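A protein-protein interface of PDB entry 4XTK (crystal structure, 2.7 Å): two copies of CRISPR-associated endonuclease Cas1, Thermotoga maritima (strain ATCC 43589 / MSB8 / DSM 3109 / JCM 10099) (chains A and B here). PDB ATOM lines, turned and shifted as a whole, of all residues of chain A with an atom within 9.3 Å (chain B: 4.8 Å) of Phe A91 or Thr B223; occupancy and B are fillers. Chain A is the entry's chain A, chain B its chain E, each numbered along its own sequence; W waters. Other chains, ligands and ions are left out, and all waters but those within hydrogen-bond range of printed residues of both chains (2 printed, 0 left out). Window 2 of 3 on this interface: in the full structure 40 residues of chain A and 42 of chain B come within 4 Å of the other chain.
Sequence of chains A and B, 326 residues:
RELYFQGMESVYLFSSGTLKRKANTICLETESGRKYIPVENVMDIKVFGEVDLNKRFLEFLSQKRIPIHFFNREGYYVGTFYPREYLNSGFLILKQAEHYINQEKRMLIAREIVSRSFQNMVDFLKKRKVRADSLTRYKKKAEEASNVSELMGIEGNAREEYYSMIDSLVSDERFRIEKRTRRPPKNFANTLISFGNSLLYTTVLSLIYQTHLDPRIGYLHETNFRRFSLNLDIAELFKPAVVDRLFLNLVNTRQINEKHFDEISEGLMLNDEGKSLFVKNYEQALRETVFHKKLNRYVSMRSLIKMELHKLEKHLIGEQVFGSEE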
ATOM      1  N   ASN A  88     -14.338 -13.534  -4.797  1.00  0.00           N
ATOM      2  CA  ASN A  88     -15.660 -12.947  -4.935  1.00  0.00           C
ATOM      3  C   ASN A  88     -15.698 -11.535  -4.387  1.00  0.00           C
ATOM      4  O   ASN A  88     -15.447 -11.296  -3.202  1.00  0.00           O
ATOM      5  CB  ASN A  88     -16.713 -13.828  -4.253  1.00  0.00           C
ATOM      6  CG  ASN A  88     -16.837 -15.199  -4.908  1.00  0.00           C
ATOM      7  OD1 ASN A  88     -17.420 -15.333  -5.983  1.00  0.00           O
ATOM      8  ND2 ASN A  88     -16.294 -16.223  -4.258  1.00  0.00           N
ATOM      9  N   SER A  89     -15.984 -10.591  -5.271  1.00  0.00           N
ATOM     10  CA  SER A  89     -16.055  -9.192  -4.884  1.00  0.00           C
ATOM     11  C   SER A  89     -17.316  -8.571  -5.450  1.00  0.00           C
ATOM     12  O   SER A  89     -17.455  -8.449  -6.665  1.00  0.00           O
ATOM     13  CB  SER A  89     -14.819  -8.439  -5.377  1.00  0.00           C
ATOM     14  OG  SER A  89     -14.860  -7.078  -4.983  1.00  0.00           O
ATOM     15  N   GLY A  90     -18.229  -8.174  -4.568  1.00  0.00           N
ATOM     16  CA  GLY A  90     -19.480  -7.579  -4.997  1.00  0.00           C
ATOM     17  C   GLY A  90     -19.234  -6.386  -5.901  1.00  0.00           C
ATOM     18  O   GLY A  90     -19.759  -6.311  -7.013  1.00  0.00           O
ATOM     19  N   PHE A  91     -18.397  -5.469  -5.427  1.00  0.00           N
ATOM     20  CA  PHE A  91     -18.167  -4.208  -6.111  1.00  0.00           C
ATOM     21  C   PHE A  91     -17.641  -4.417  -7.524  1.00  0.00           C
ATOM     22  O   PHE A  91     -18.184  -3.872  -8.483  1.00  0.00           O
ATOM     23  CB  PHE A  91     -17.190  -3.352  -5.309  1.00  0.00           C
ATOM     24  CG  PHE A  91     -17.178  -1.905  -5.710  1.00  0.00           C
ATOM     25  CD1 PHE A  91     -18.219  -1.063  -5.354  1.00  0.00           C
ATOM     26  CD2 PHE A  91     -16.120  -1.384  -6.438  1.00  0.00           C
ATOM     27  CE1 PHE A  91     -18.197   0.280  -5.714  1.00  0.00           C
ATOM     28  CE2 PHE A  91     -16.101  -0.046  -6.803  1.00  0.00           C
ATOM     29  CZ  PHE A  91     -17.138   0.781  -6.435  1.00  0.00           C
ATOM     30  N   LEU A  92     -16.592  -5.222  -7.652  1.00  0.00           N
ATOM     31  CA  LEU A  92     -15.948  -5.397  -8.946  1.00  0.00           C
ATOM     32  C   LEU A  92     -16.861  -6.074  -9.978  1.00  0.00           C
ATOM     33  O   LEU A  92     -16.906  -5.652 -11.131  1.00  0.00           O
ATOM     34  CB  LEU A  92     -14.653  -6.186  -8.787  1.00  0.00           C
ATOM     35  CG  LEU A  92     -13.893  -6.257 -10.107  1.00  0.00           C
ATOM     36  CD1 LEU A  92     -12.491  -5.755  -9.907  1.00  0.00           C
ATOM     37  CD2 LEU A  92     -13.903  -7.680 -10.655  1.00  0.00           C
ATOM     38  N   ILE A  93     -17.581  -7.114  -9.565  1.00  0.00           N
ATOM     39  CA  ILE A  93     -18.586  -7.738 -10.422  1.00  0.00           C
ATOM     40  C   ILE A  93     -19.643  -6.717 -10.848  1.00  0.00           C
ATOM     41  O   ILE A  93     -20.078  -6.689 -12.005  1.00  0.00           O
ATOM     42  CB  ILE A  93     -19.265  -8.928  -9.711  1.00  0.00           C
ATOM     43  CG1 ILE A  93     -18.274 -10.082  -9.577  1.00  0.00           C
ATOM     44  CG2 ILE A  93     -20.483  -9.410 -10.482  1.00  0.00           C
ATOM     45  CD1 ILE A  93     -17.749 -10.582 -10.906  1.00  0.00           C
ATOM     46  N   LEU A  94     -20.045  -5.868  -9.910  1.00  0.00           N
ATOM     47  CA  LEU A  94     -21.018  -4.828 -10.206  1.00  0.00           C
ATOM     48  C   LEU A  94     -20.456  -3.869 -11.242  1.00  0.00           C
ATOM     49  O   LEU A  94     -21.152  -3.467 -12.180  1.00  0.00           O
ATOM     50  CB  LEU A  94     -21.405  -4.076  -8.932  1.00  0.00           C
ATOM     51  CG  LEU A  94     -22.285  -2.839  -9.113  1.00  0.00           C
ATOM     52  CD1 LEU A  94     -23.696  -3.248  -9.508  1.00  0.00           C
ATOM     53  CD2 LEU A  94     -22.293  -2.000  -7.847  1.00  0.00           C
ATOM     54  N   LYS A  95     -19.186  -3.511 -11.073  1.00  0.00           N
ATOM     55  CA  LYS A  95     -18.523  -2.608 -12.006  1.00  0.00           C
ATOM     56  C   LYS A  95     -18.330  -3.264 -13.363  1.00  0.00           C
ATOM     57  O   LYS A  95     -18.534  -2.626 -14.390  1.00  0.00           O
ATOM     58  CB  LYS A  95     -17.177  -2.138 -11.452  1.00  0.00           C
ATOM     59  CG  LYS A  95     -17.317  -1.192 -10.271  1.00  0.00           C
ATOM     60  CD  LYS A  95     -18.179  -0.003 -10.649  1.00  0.00           C
ATOM     61  CE  LYS A  95     -18.728   0.695  -9.421  1.00  0.00           C
ATOM     62  NZ  LYS A  95     -19.889   1.574  -9.743  1.00  0.00           N
ATOM     63  N   GLN A  96     -17.952  -4.540 -13.370  1.00  0.00           N
ATOM     64  CA  GLN A  96     -17.776  -5.258 -14.625  1.00  0.00           C
ATOM     65  C   GLN A  96     -19.073  -5.235 -15.429  1.00  0.00           C
ATOM     66  O   GLN A  96     -19.049  -5.080 -16.645  1.00  0.00           O
ATOM     67  CB  GLN A  96     -17.319  -6.702 -14.381  1.00  0.00           C
ATOM     68  CG  GLN A  96     -16.947  -7.449 -15.668  1.00  0.00           C
ATOM     69  CD  GLN A  96     -16.373  -8.836 -15.422  1.00  0.00           C
ATOM     70  OE1 GLN A  96     -16.365  -9.330 -14.295  1.00  0.00           O
ATOM     71  NE2 GLN A  96     -15.887  -9.469 -16.485  1.00  0.00           N
ATOM     72  N   ALA A  97     -20.208  -5.356 -14.748  1.00  0.00           N
ATOM     73  CA  ALA A  97     -21.494  -5.379 -15.445  1.00  0.00           C
ATOM     74  C   ALA A  97     -21.968  -3.989 -15.862  1.00  0.00           C
ATOM     75  O   ALA A  97     -22.498  -3.814 -16.961  1.00  0.00           O
ATOM     76  CB  ALA A  97     -22.557  -6.055 -14.585  1.00  0.00           C
ATOM     77  N   GLU A  98     -21.790  -2.998 -14.991  1.00  0.00           N
ATOM     78  CA  GLU A  98     -22.278  -1.667 -15.309  1.00  0.00           C
ATOM     79  C   GLU A  98     -21.403  -1.051 -16.401  1.00  0.00           C
ATOM     80  O   GLU A  98     -21.837  -0.162 -17.132  1.00  0.00           O
ATOM     81  CB  GLU A  98     -22.328  -0.784 -14.057  1.00  0.00           C
ATOM     82  CG  GLU A  98     -21.163   0.174 -13.887  1.00  0.00           C
ATOM     83  CD  GLU A  98     -21.320   1.059 -12.660  1.00  0.00           C
ATOM     84  OE1 GLU A  98     -21.858   0.570 -11.638  1.00  0.00           O
ATOM     85  OE2 GLU A  98     -20.906   2.241 -12.720  1.00  0.00           O
ATOM     86  N   HIS A  99     -20.180  -1.550 -16.526  1.00  0.00           N
ATOM     87  CA  HIS A  99     -19.301  -1.113 -17.596  1.00  0.00           C
ATOM     88  C   HIS A  99     -19.704  -1.754 -18.918  1.00  0.00           C
ATOM     89  O   HIS A  99     -19.357  -1.253 -19.987  1.00  0.00           O
ATOM     90  CB  HIS A  99     -17.844  -1.436 -17.271  1.00  0.00           C
ATOM     91  CG  HIS A  99     -17.156  -0.366 -16.485  1.00  0.00           C
ATOM     92  ND1 HIS A  99     -16.477   0.674 -17.084  1.00  0.00           N
ATOM     93  CD2 HIS A  99     -17.046  -0.168 -15.150  1.00  0.00           C
ATOM     94  CE1 HIS A  99     -15.973   1.462 -16.151  1.00  0.00           C
ATOM     95  NE2 HIS A  99     -16.305   0.972 -14.969  1.00  0.00           N
ATOM     96  N   HIS A 212     -10.863 -11.589  -9.747  1.00  0.00           N
ATOM     97  CA  HIS A 212     -12.233 -11.369  -9.305  1.00  0.00           C
ATOM     98  C   HIS A 212     -13.194 -11.173 -10.471  1.00  0.00           C
ATOM     99  O   HIS A 212     -14.397 -10.991 -10.265  1.00  0.00           O
ATOM    100  CB  HIS A 212     -12.308 -10.164  -8.369  1.00  0.00           C
ATOM    101  CG  HIS A 212     -11.538 -10.341  -7.100  1.00  0.00           C
ATOM    102  ND1 HIS A 212     -12.146 -10.498  -5.876  1.00  0.00           N
ATOM    103  CD2 HIS A 212     -10.202 -10.376  -6.868  1.00  0.00           C
ATOM    104  CE1 HIS A 212     -11.223 -10.637  -4.942  1.00  0.00           C
ATOM    105  NE2 HIS A 212     -10.035 -10.563  -5.515  1.00  0.00           N
ATOM    106  N   LEU A 213     -12.661 -11.205 -11.690  1.00  0.00           N
ATOM    107  CA  LEU A 213     -13.470 -11.005 -12.892  1.00  0.00           C
ATOM    108  C   LEU A 213     -14.297 -12.228 -13.269  1.00  0.00           C
ATOM    109  O   LEU A 213     -13.875 -13.369 -13.069  1.00  0.00           O
ATOM    110  CB  LEU A 213     -12.579 -10.629 -14.075  1.00  0.00           C
ATOM    111  CG  LEU A 213     -11.839  -9.297 -14.038  1.00  0.00           C
ATOM    112  CD1 LEU A 213     -10.639  -9.321 -14.986  1.00  0.00           C
ATOM    113  CD2 LEU A 213     -12.788  -8.167 -14.390  1.00  0.00           C
ATOM    114  N   GLU A 313      -9.234  -4.569 -14.059  1.00  0.00           N
ATOM    115  CA  GLU A 313      -9.901  -4.461 -12.769  1.00  0.00           C
ATOM    116  C   GLU A 313      -9.692  -3.087 -12.144  1.00  0.00           C
ATOM    117  O   GLU A 313     -10.638  -2.468 -11.653  1.00  0.00           O
ATOM    118  CB  GLU A 313      -9.411  -5.553 -11.827  1.00  0.00           C
ATOM    119  CG  GLU A 313      -9.944  -6.929 -12.177  1.00  0.00           C
ATOM    120  CD  GLU A 313      -9.560  -7.987 -11.165  1.00  0.00           C
ATOM    121  OE1 GLU A 313      -8.379  -8.027 -10.763  1.00  0.00           O
ATOM    122  OE2 GLU A 313     -10.443  -8.777 -10.772  1.00  0.00           O
ATOM    123  N   LYS A 314      -8.451  -2.612 -12.168  1.00  0.00           N
ATOM    124  CA  LYS A 314      -8.137  -1.262 -11.714  1.00  0.00           C
ATOM    125  C   LYS A 314      -8.978  -0.235 -12.464  1.00  0.00           C
ATOM    126  O   LYS A 314      -9.453   0.742 -11.880  1.00  0.00           O
ATOM    127  CB  LYS A 314      -6.655  -0.957 -11.904  1.00  0.00           C
ATOM    128  CG  LYS A 314      -5.726  -1.736 -10.996  1.00  0.00           C
ATOM    129  CD  LYS A 314      -4.280  -1.398 -11.316  1.00  0.00           C
ATOM    130  CE  LYS A 314      -3.311  -2.214 -10.484  1.00  0.00           C
ATOM    131  NZ  LYS A 314      -1.912  -2.025 -10.956  1.00  0.00           N
ATOM    132  N   HIS A 315      -9.170  -0.479 -13.758  1.00  0.00           N
ATOM    133  CA  HIS A 315      -9.979   0.394 -14.600  1.00  0.00           C
ATOM    134  C   HIS A 315     -11.450   0.385 -14.208  1.00  0.00           C
ATOM    135  O   HIS A 315     -12.083   1.435 -14.143  1.00  0.00           O
ATOM    136  CB  HIS A 315      -9.855  -0.004 -16.073  1.00  0.00           C
ATOM    137  CG  HIS A 315     -10.765   0.767 -16.979  1.00  0.00           C
ATOM    138  ND1 HIS A 315     -10.504   2.062 -17.368  1.00  0.00           N
ATOM    139  CD2 HIS A 315     -11.945   0.433 -17.552  1.00  0.00           C
ATOM    140  CE1 HIS A 315     -11.476   2.488 -18.152  1.00  0.00           C
ATOM    141  NE2 HIS A 315     -12.366   1.521 -18.280  1.00  0.00           N
ATOM    142  N   LEU A 316     -11.995  -0.803 -13.968  1.00  0.00           N
ATOM    143  CA  LEU A 316     -13.419  -0.939 -13.666  1.00  0.00           C
ATOM    144  C   LEU A 316     -13.794  -0.191 -12.390  1.00  0.00           C
ATOM    145  O   LEU A 316     -14.910   0.310 -12.262  1.00  0.00           O
ATOM    146  CB  LEU A 316     -13.806  -2.419 -13.546  1.00  0.00           C
ATOM    147  CG  LEU A 316     -13.747  -3.273 -14.826  1.00  0.00           C
ATOM    148  CD1 LEU A 316     -14.047  -4.738 -14.533  1.00  0.00           C
ATOM    149  CD2 LEU A 316     -14.690  -2.754 -15.898  1.00  0.00           C
ATOM    150  N   ILE A 317     -12.858  -0.120 -11.448  1.00  0.00           N
ATOM    151  CA  ILE A 317     -13.106   0.537 -10.172  1.00  0.00           C
ATOM    152  C   ILE A 317     -12.581   1.974 -10.103  1.00  0.00           C
ATOM    153  O   ILE A 317     -12.666   2.623  -9.051  1.00  0.00           O
ATOM    154  CB  ILE A 317     -12.501  -0.265  -9.014  1.00  0.00           C
ATOM    155  CG1 ILE A 317     -10.975  -0.197  -9.060  1.00  0.00           C
ATOM    156  CG2 ILE A 317     -13.006  -1.707  -9.053  1.00  0.00           C
ATOM    157  CD1 ILE A 317     -10.309  -0.775  -7.833  1.00  0.00           C
ATOM    158  N   GLY A 318     -12.021   2.466 -11.205  1.00  0.00           N
ATOM    159  CA  GLY A 318     -11.696   3.880 -11.304  1.00  0.00           C
ATOM    160  C   GLY A 318     -10.234   4.263 -11.230  1.00  0.00           C
ATOM    161  O   GLY A 318      -9.886   5.414 -11.483  1.00  0.00           O
ATOM    162  N   GLU A 319      -9.371   3.325 -10.860  1.00  0.00           N
ATOM    163  CA  GLU A 319      -7.934   3.579 -10.926  1.00  0.00           C
ATOM    164  C   GLU A 319      -7.468   3.520 -12.369  1.00  0.00           C
ATOM    165  O   GLU A 319      -8.159   2.951 -13.216  1.00  0.00           O
ATOM    166  CB  GLU A 319      -7.137   2.567 -10.106  1.00  0.00           C
ATOM    167  CG  GLU A 319      -7.476   2.493  -8.639  1.00  0.00           C
ATOM    168  CD  GLU A 319      -6.649   1.433  -7.931  1.00  0.00           C
ATOM    169  OE1 GLU A 319      -5.866   0.741  -8.616  1.00  0.00           O
ATOM    170  OE2 GLU A 319      -6.774   1.293  -6.697  1.00  0.00           O
ATOM    171  N   TYR B 100     -29.498  -2.292  -9.775  1.00  0.00           N
ATOM    172  CA  TYR B 100     -28.766  -1.718  -8.667  1.00  0.00           C
ATOM    173  C   TYR B 100     -28.395  -0.234  -8.868  1.00  0.00           C
ATOM    174  O   TYR B 100     -28.571   0.575  -7.956  1.00  0.00           O
ATOM    175  CB  TYR B 100     -27.506  -2.523  -8.393  1.00  0.00           C
ATOM    176  CG  TYR B 100     -26.794  -2.078  -7.138  1.00  0.00           C
ATOM    177  CD1 TYR B 100     -27.177  -2.560  -5.892  1.00  0.00           C
ATOM    178  CD2 TYR B 100     -25.751  -1.155  -7.193  1.00  0.00           C
ATOM    179  CE1 TYR B 100     -26.539  -2.151  -4.745  1.00  0.00           C
ATOM    180  CE2 TYR B 100     -25.104  -0.741  -6.040  1.00  0.00           C
ATOM    181  CZ  TYR B 100     -25.503  -1.245  -4.822  1.00  0.00           C
ATOM    182  OH  TYR B 100     -24.865  -0.840  -3.674  1.00  0.00           O
ATOM    183  N   ARG B 216     -23.441 -11.990  -5.832  1.00  0.00           N
ATOM    184  CA  ARG B 216     -22.524 -10.901  -5.489  1.00  0.00           C
ATOM    185  C   ARG B 216     -23.155  -9.516  -5.565  1.00  0.00           C
ATOM    186  O   ARG B 216     -22.568  -8.546  -5.103  1.00  0.00           O
ATOM    187  CB  ARG B 216     -21.287 -10.953  -6.379  1.00  0.00           C
ATOM    188  CG  ARG B 216     -20.403 -12.124  -6.028  1.00  0.00           C
ATOM    189  CD  ARG B 216     -19.368 -12.399  -7.082  1.00  0.00           C
ATOM    190  NE  ARG B 216     -19.964 -12.791  -8.351  1.00  0.00           N
ATOM    191  CZ  ARG B 216     -19.269 -13.328  -9.346  1.00  0.00           C
ATOM    192  NH1 ARG B 216     -17.967 -13.546  -9.194  1.00  0.00           N
ATOM    193  NH2 ARG B 216     -19.867 -13.654 -10.483  1.00  0.00           N
ATOM    194  N   ILE B 217     -24.352  -9.423  -6.126  1.00  0.00           N
ATOM    195  CA  ILE B 217     -25.057  -8.151  -6.147  1.00  0.00           C
ATOM    196  C   ILE B 217     -26.317  -8.208  -5.299  1.00  0.00           C
ATOM    197  O   ILE B 217     -27.251  -8.922  -5.631  1.00  0.00           O
ATOM    198  CB  ILE B 217     -25.428  -7.725  -7.588  1.00  0.00           C
ATOM    199  CG1 ILE B 217     -24.167  -7.545  -8.432  1.00  0.00           C
ATOM    200  CG2 ILE B 217     -26.239  -6.451  -7.573  1.00  0.00           C
ATOM    201  CD1 ILE B 217     -24.449  -7.190  -9.869  1.00  0.00           C
ATOM    202  N   GLY B 218     -26.327  -7.457  -4.200  1.00  0.00           N
ATOM    203  CA  GLY B 218     -27.510  -7.292  -3.371  1.00  0.00           C
ATOM    204  C   GLY B 218     -28.172  -5.925  -3.521  1.00  0.00           C
ATOM    205  O   GLY B 218     -27.727  -5.096  -4.314  1.00  0.00           O
ATOM    206  N   HIS B 221     -28.727  -4.602   1.178  1.00  0.00           N
ATOM    207  CA  HIS B 221     -27.320  -4.443   1.524  1.00  0.00           C
ATOM    208  C   HIS B 221     -26.569  -3.765   0.391  1.00  0.00           C
ATOM    209  O   HIS B 221     -26.840  -4.010  -0.786  1.00  0.00           O
ATOM    210  CB  HIS B 221     -26.683  -5.793   1.846  1.00  0.00           C
ATOM    211  CG  HIS B 221     -27.252  -6.447   3.062  1.00  0.00           C
ATOM    212  ND1 HIS B 221     -28.494  -7.039   3.078  1.00  0.00           N
ATOM    213  CD2 HIS B 221     -26.760  -6.575   4.322  1.00  0.00           C
ATOM    214  CE1 HIS B 221     -28.741  -7.520   4.285  1.00  0.00           C
ATOM    215  NE2 HIS B 221     -27.703  -7.242   5.057  1.00  0.00           N
ATOM    216  N   GLU B 222     -25.628  -2.902   0.749  1.00  0.00           N
ATOM    217  CA  GLU B 222     -24.791  -2.248  -0.242  1.00  0.00           C
ATOM    218  C   GLU B 222     -23.960  -3.290  -0.988  1.00  0.00           C
ATOM    219  O   GLU B 222     -23.404  -4.199  -0.376  1.00  0.00           O
ATOM    220  CB  GLU B 222     -23.884  -1.211   0.430  1.00  0.00           C
ATOM    221  CG  GLU B 222     -23.246  -0.223  -0.531  1.00  0.00           C
ATOM    222  CD  GLU B 222     -22.153   0.613   0.117  1.00  0.00           C
ATOM    223  OE1 GLU B 222     -20.963   0.342  -0.147  1.00  0.00           O
ATOM    224  OE2 GLU B 222     -22.482   1.539   0.888  1.00  0.00           O
ATOM    225  N   THR B 223     -23.851  -3.158  -2.304  1.00  0.00           N
ATOM    226  CA  THR B 223     -22.975  -4.067  -3.017  1.00  0.00           C
ATOM    227  C   THR B 223     -21.605  -3.411  -2.986  1.00  0.00           C
ATOM    228  O   THR B 223     -21.353  -2.409  -3.649  1.00  0.00           O
ATOM    229  CB  THR B 223     -23.434  -4.336  -4.468  1.00  0.00           C
ATOM    230  OG1 THR B 223     -24.722  -4.960  -4.455  1.00  0.00           O
ATOM    231  CG2 THR B 223     -22.448  -5.261  -5.192  1.00  0.00           C
ATOM    232  N   ASN B 224     -20.726  -4.025  -2.207  1.00  0.00           N
ATOM    233  CA  ASN B 224     -19.429  -3.479  -1.847  1.00  0.00           C
ATOM    234  C   ASN B 224     -18.451  -4.639  -1.913  1.00  0.00           C
ATOM    235  O   ASN B 224     -18.733  -5.633  -2.573  1.00  0.00           O
ATOM    236  CB  ASN B 224     -19.435  -2.799  -0.470  1.00  0.00           C
ATOM    237  CG  ASN B 224     -19.944  -3.697   0.637  1.00  0.00           C
ATOM    238  OD1 ASN B 224     -19.979  -4.915   0.501  1.00  0.00           O
ATOM    239  ND2 ASN B 224     -20.336  -3.090   1.750  1.00  0.00           N
ATOM    240  N   PHE B 225     -17.287  -4.503  -1.292  1.00  0.00           N
ATOM    241  CA  PHE B 225     -16.222  -5.479  -1.491  1.00  0.00           C
ATOM    242  C   PHE B 225     -16.429  -6.758  -0.689  1.00  0.00           C
ATOM    243  O   PHE B 225     -15.584  -7.651  -0.680  1.00  0.00           O
ATOM    244  CB  PHE B 225     -14.880  -4.837  -1.177  1.00  0.00           C
ATOM    245  CG  PHE B 225     -14.402  -3.944  -2.273  1.00  0.00           C
ATOM    246  CD1 PHE B 225     -14.933  -2.678  -2.424  1.00  0.00           C
ATOM    247  CD2 PHE B 225     -13.460  -4.388  -3.185  1.00  0.00           C
ATOM    248  CE1 PHE B 225     -14.513  -1.860  -3.444  1.00  0.00           C
ATOM    249  CE2 PHE B 225     -13.035  -3.574  -4.207  1.00  0.00           C
ATOM    250  CZ  PHE B 225     -13.563  -2.309  -4.338  1.00  0.00           C
ATOM    251  N   SER B 229     -23.837 -10.618  -1.143  1.00  0.00           N
ATOM    252  CA  SER B 229     -24.790  -9.619  -0.654  1.00  0.00           C
ATOM    253  C   SER B 229     -26.225 -10.124  -0.763  1.00  0.00           C
ATOM    254  O   SER B 229     -26.996 -10.064   0.201  1.00  0.00           O
ATOM    255  CB  SER B 229     -24.641  -8.292  -1.411  1.00  0.00           C
ATOM    256  OG  SER B 229     -23.455  -7.618  -1.030  1.00  0.00           O
HETATM  257  O   HOH W   1     -15.660 -11.555  -7.701  1.00  0.00           O
HETATM  258  O   HOH W   2     -13.351  -9.052  -2.281  1.00  0.00           O
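The side-chain hydroxyl (OH) of Tyr B100 lies within hydrogen-bond range of the backbone NH (N) of Thr B223. N of Gly B218 is in hydrogen-bond range of OG1 of Thr B223 (3.0 Å).
Water W1 lies within hydrogen-bond range of N of Ser A89 (2.6 Å), O of His A212 (2.9 Å) and NH1 of Arg B216 (3.4 Å). Water W2 bridges O of Phe B225 and O of Asn A88.
Phe A91 touches three residues of chain B. Of the printed residues of chain A, Thr B223 touches Gly A90 (3.4 Å) and Phe A91 (3.8 Å). Gly B218 touches none of the printed residues of chain A. Of the printed residues of chain A, Asn B224 touches Gly A90 (3.2 Å) and Phe A91 (2.9 Å). Of the printed residues of chain A, Phe B225 touches Ser A89 (3.5 Å) and Phe A91 (3.4 Å). Printed residues of chain B within 4 Å of Leu A94: Tyr B100 (3.6 Å). His A99 touches none of the printed residues of chain B. The nearest residue of chain A that does not touch Thr B223 is Leu A94 (4.1 Å). The nearest printed residue of chain A that does not touch Tyr B100 is Glu A98 (6.2 Å).
No position is printed for both chains.
The backbone NH (N) of Gly A90 sits close to the backbone carbonyl oxygen (O) of Asn B224, 3.3 Å away. The backbone NH (N) of Phe A91 is in hydrogen-bond range of the backbone carbonyl oxygen (O) of Asn B224, at 2.9 Å.
Of the 21 printed residues of chain A, 6 touch a printed residue of chain B. Hydrophobic or aromatic side chains of chain A that line the printed part of chain B: Phe A91, Ile A93 and Leu A94. Along chain A the printed residues that touch a printed residue of chain B span positions 88 to 94. Along chain B the printed residues that touch a printed residue of chain A span positions 100 to 225.
Asn A88 touches Arg B216 (OD1 to CD, 3.7 Å). Ser A89 touches Phe B225. Gly A90 touches Arg B216. O of Gly A90 touches CG2 of Thr B223, 3.4 Å away. Phe A91 touches Thr B223. Phe A91 touches Phe B225. CZ of Arg B216 touches CG1 of Ile A93, at 3.4 Å. CD2 of Leu A94 touches CE2 of Tyr B100, 3.6 Å away.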
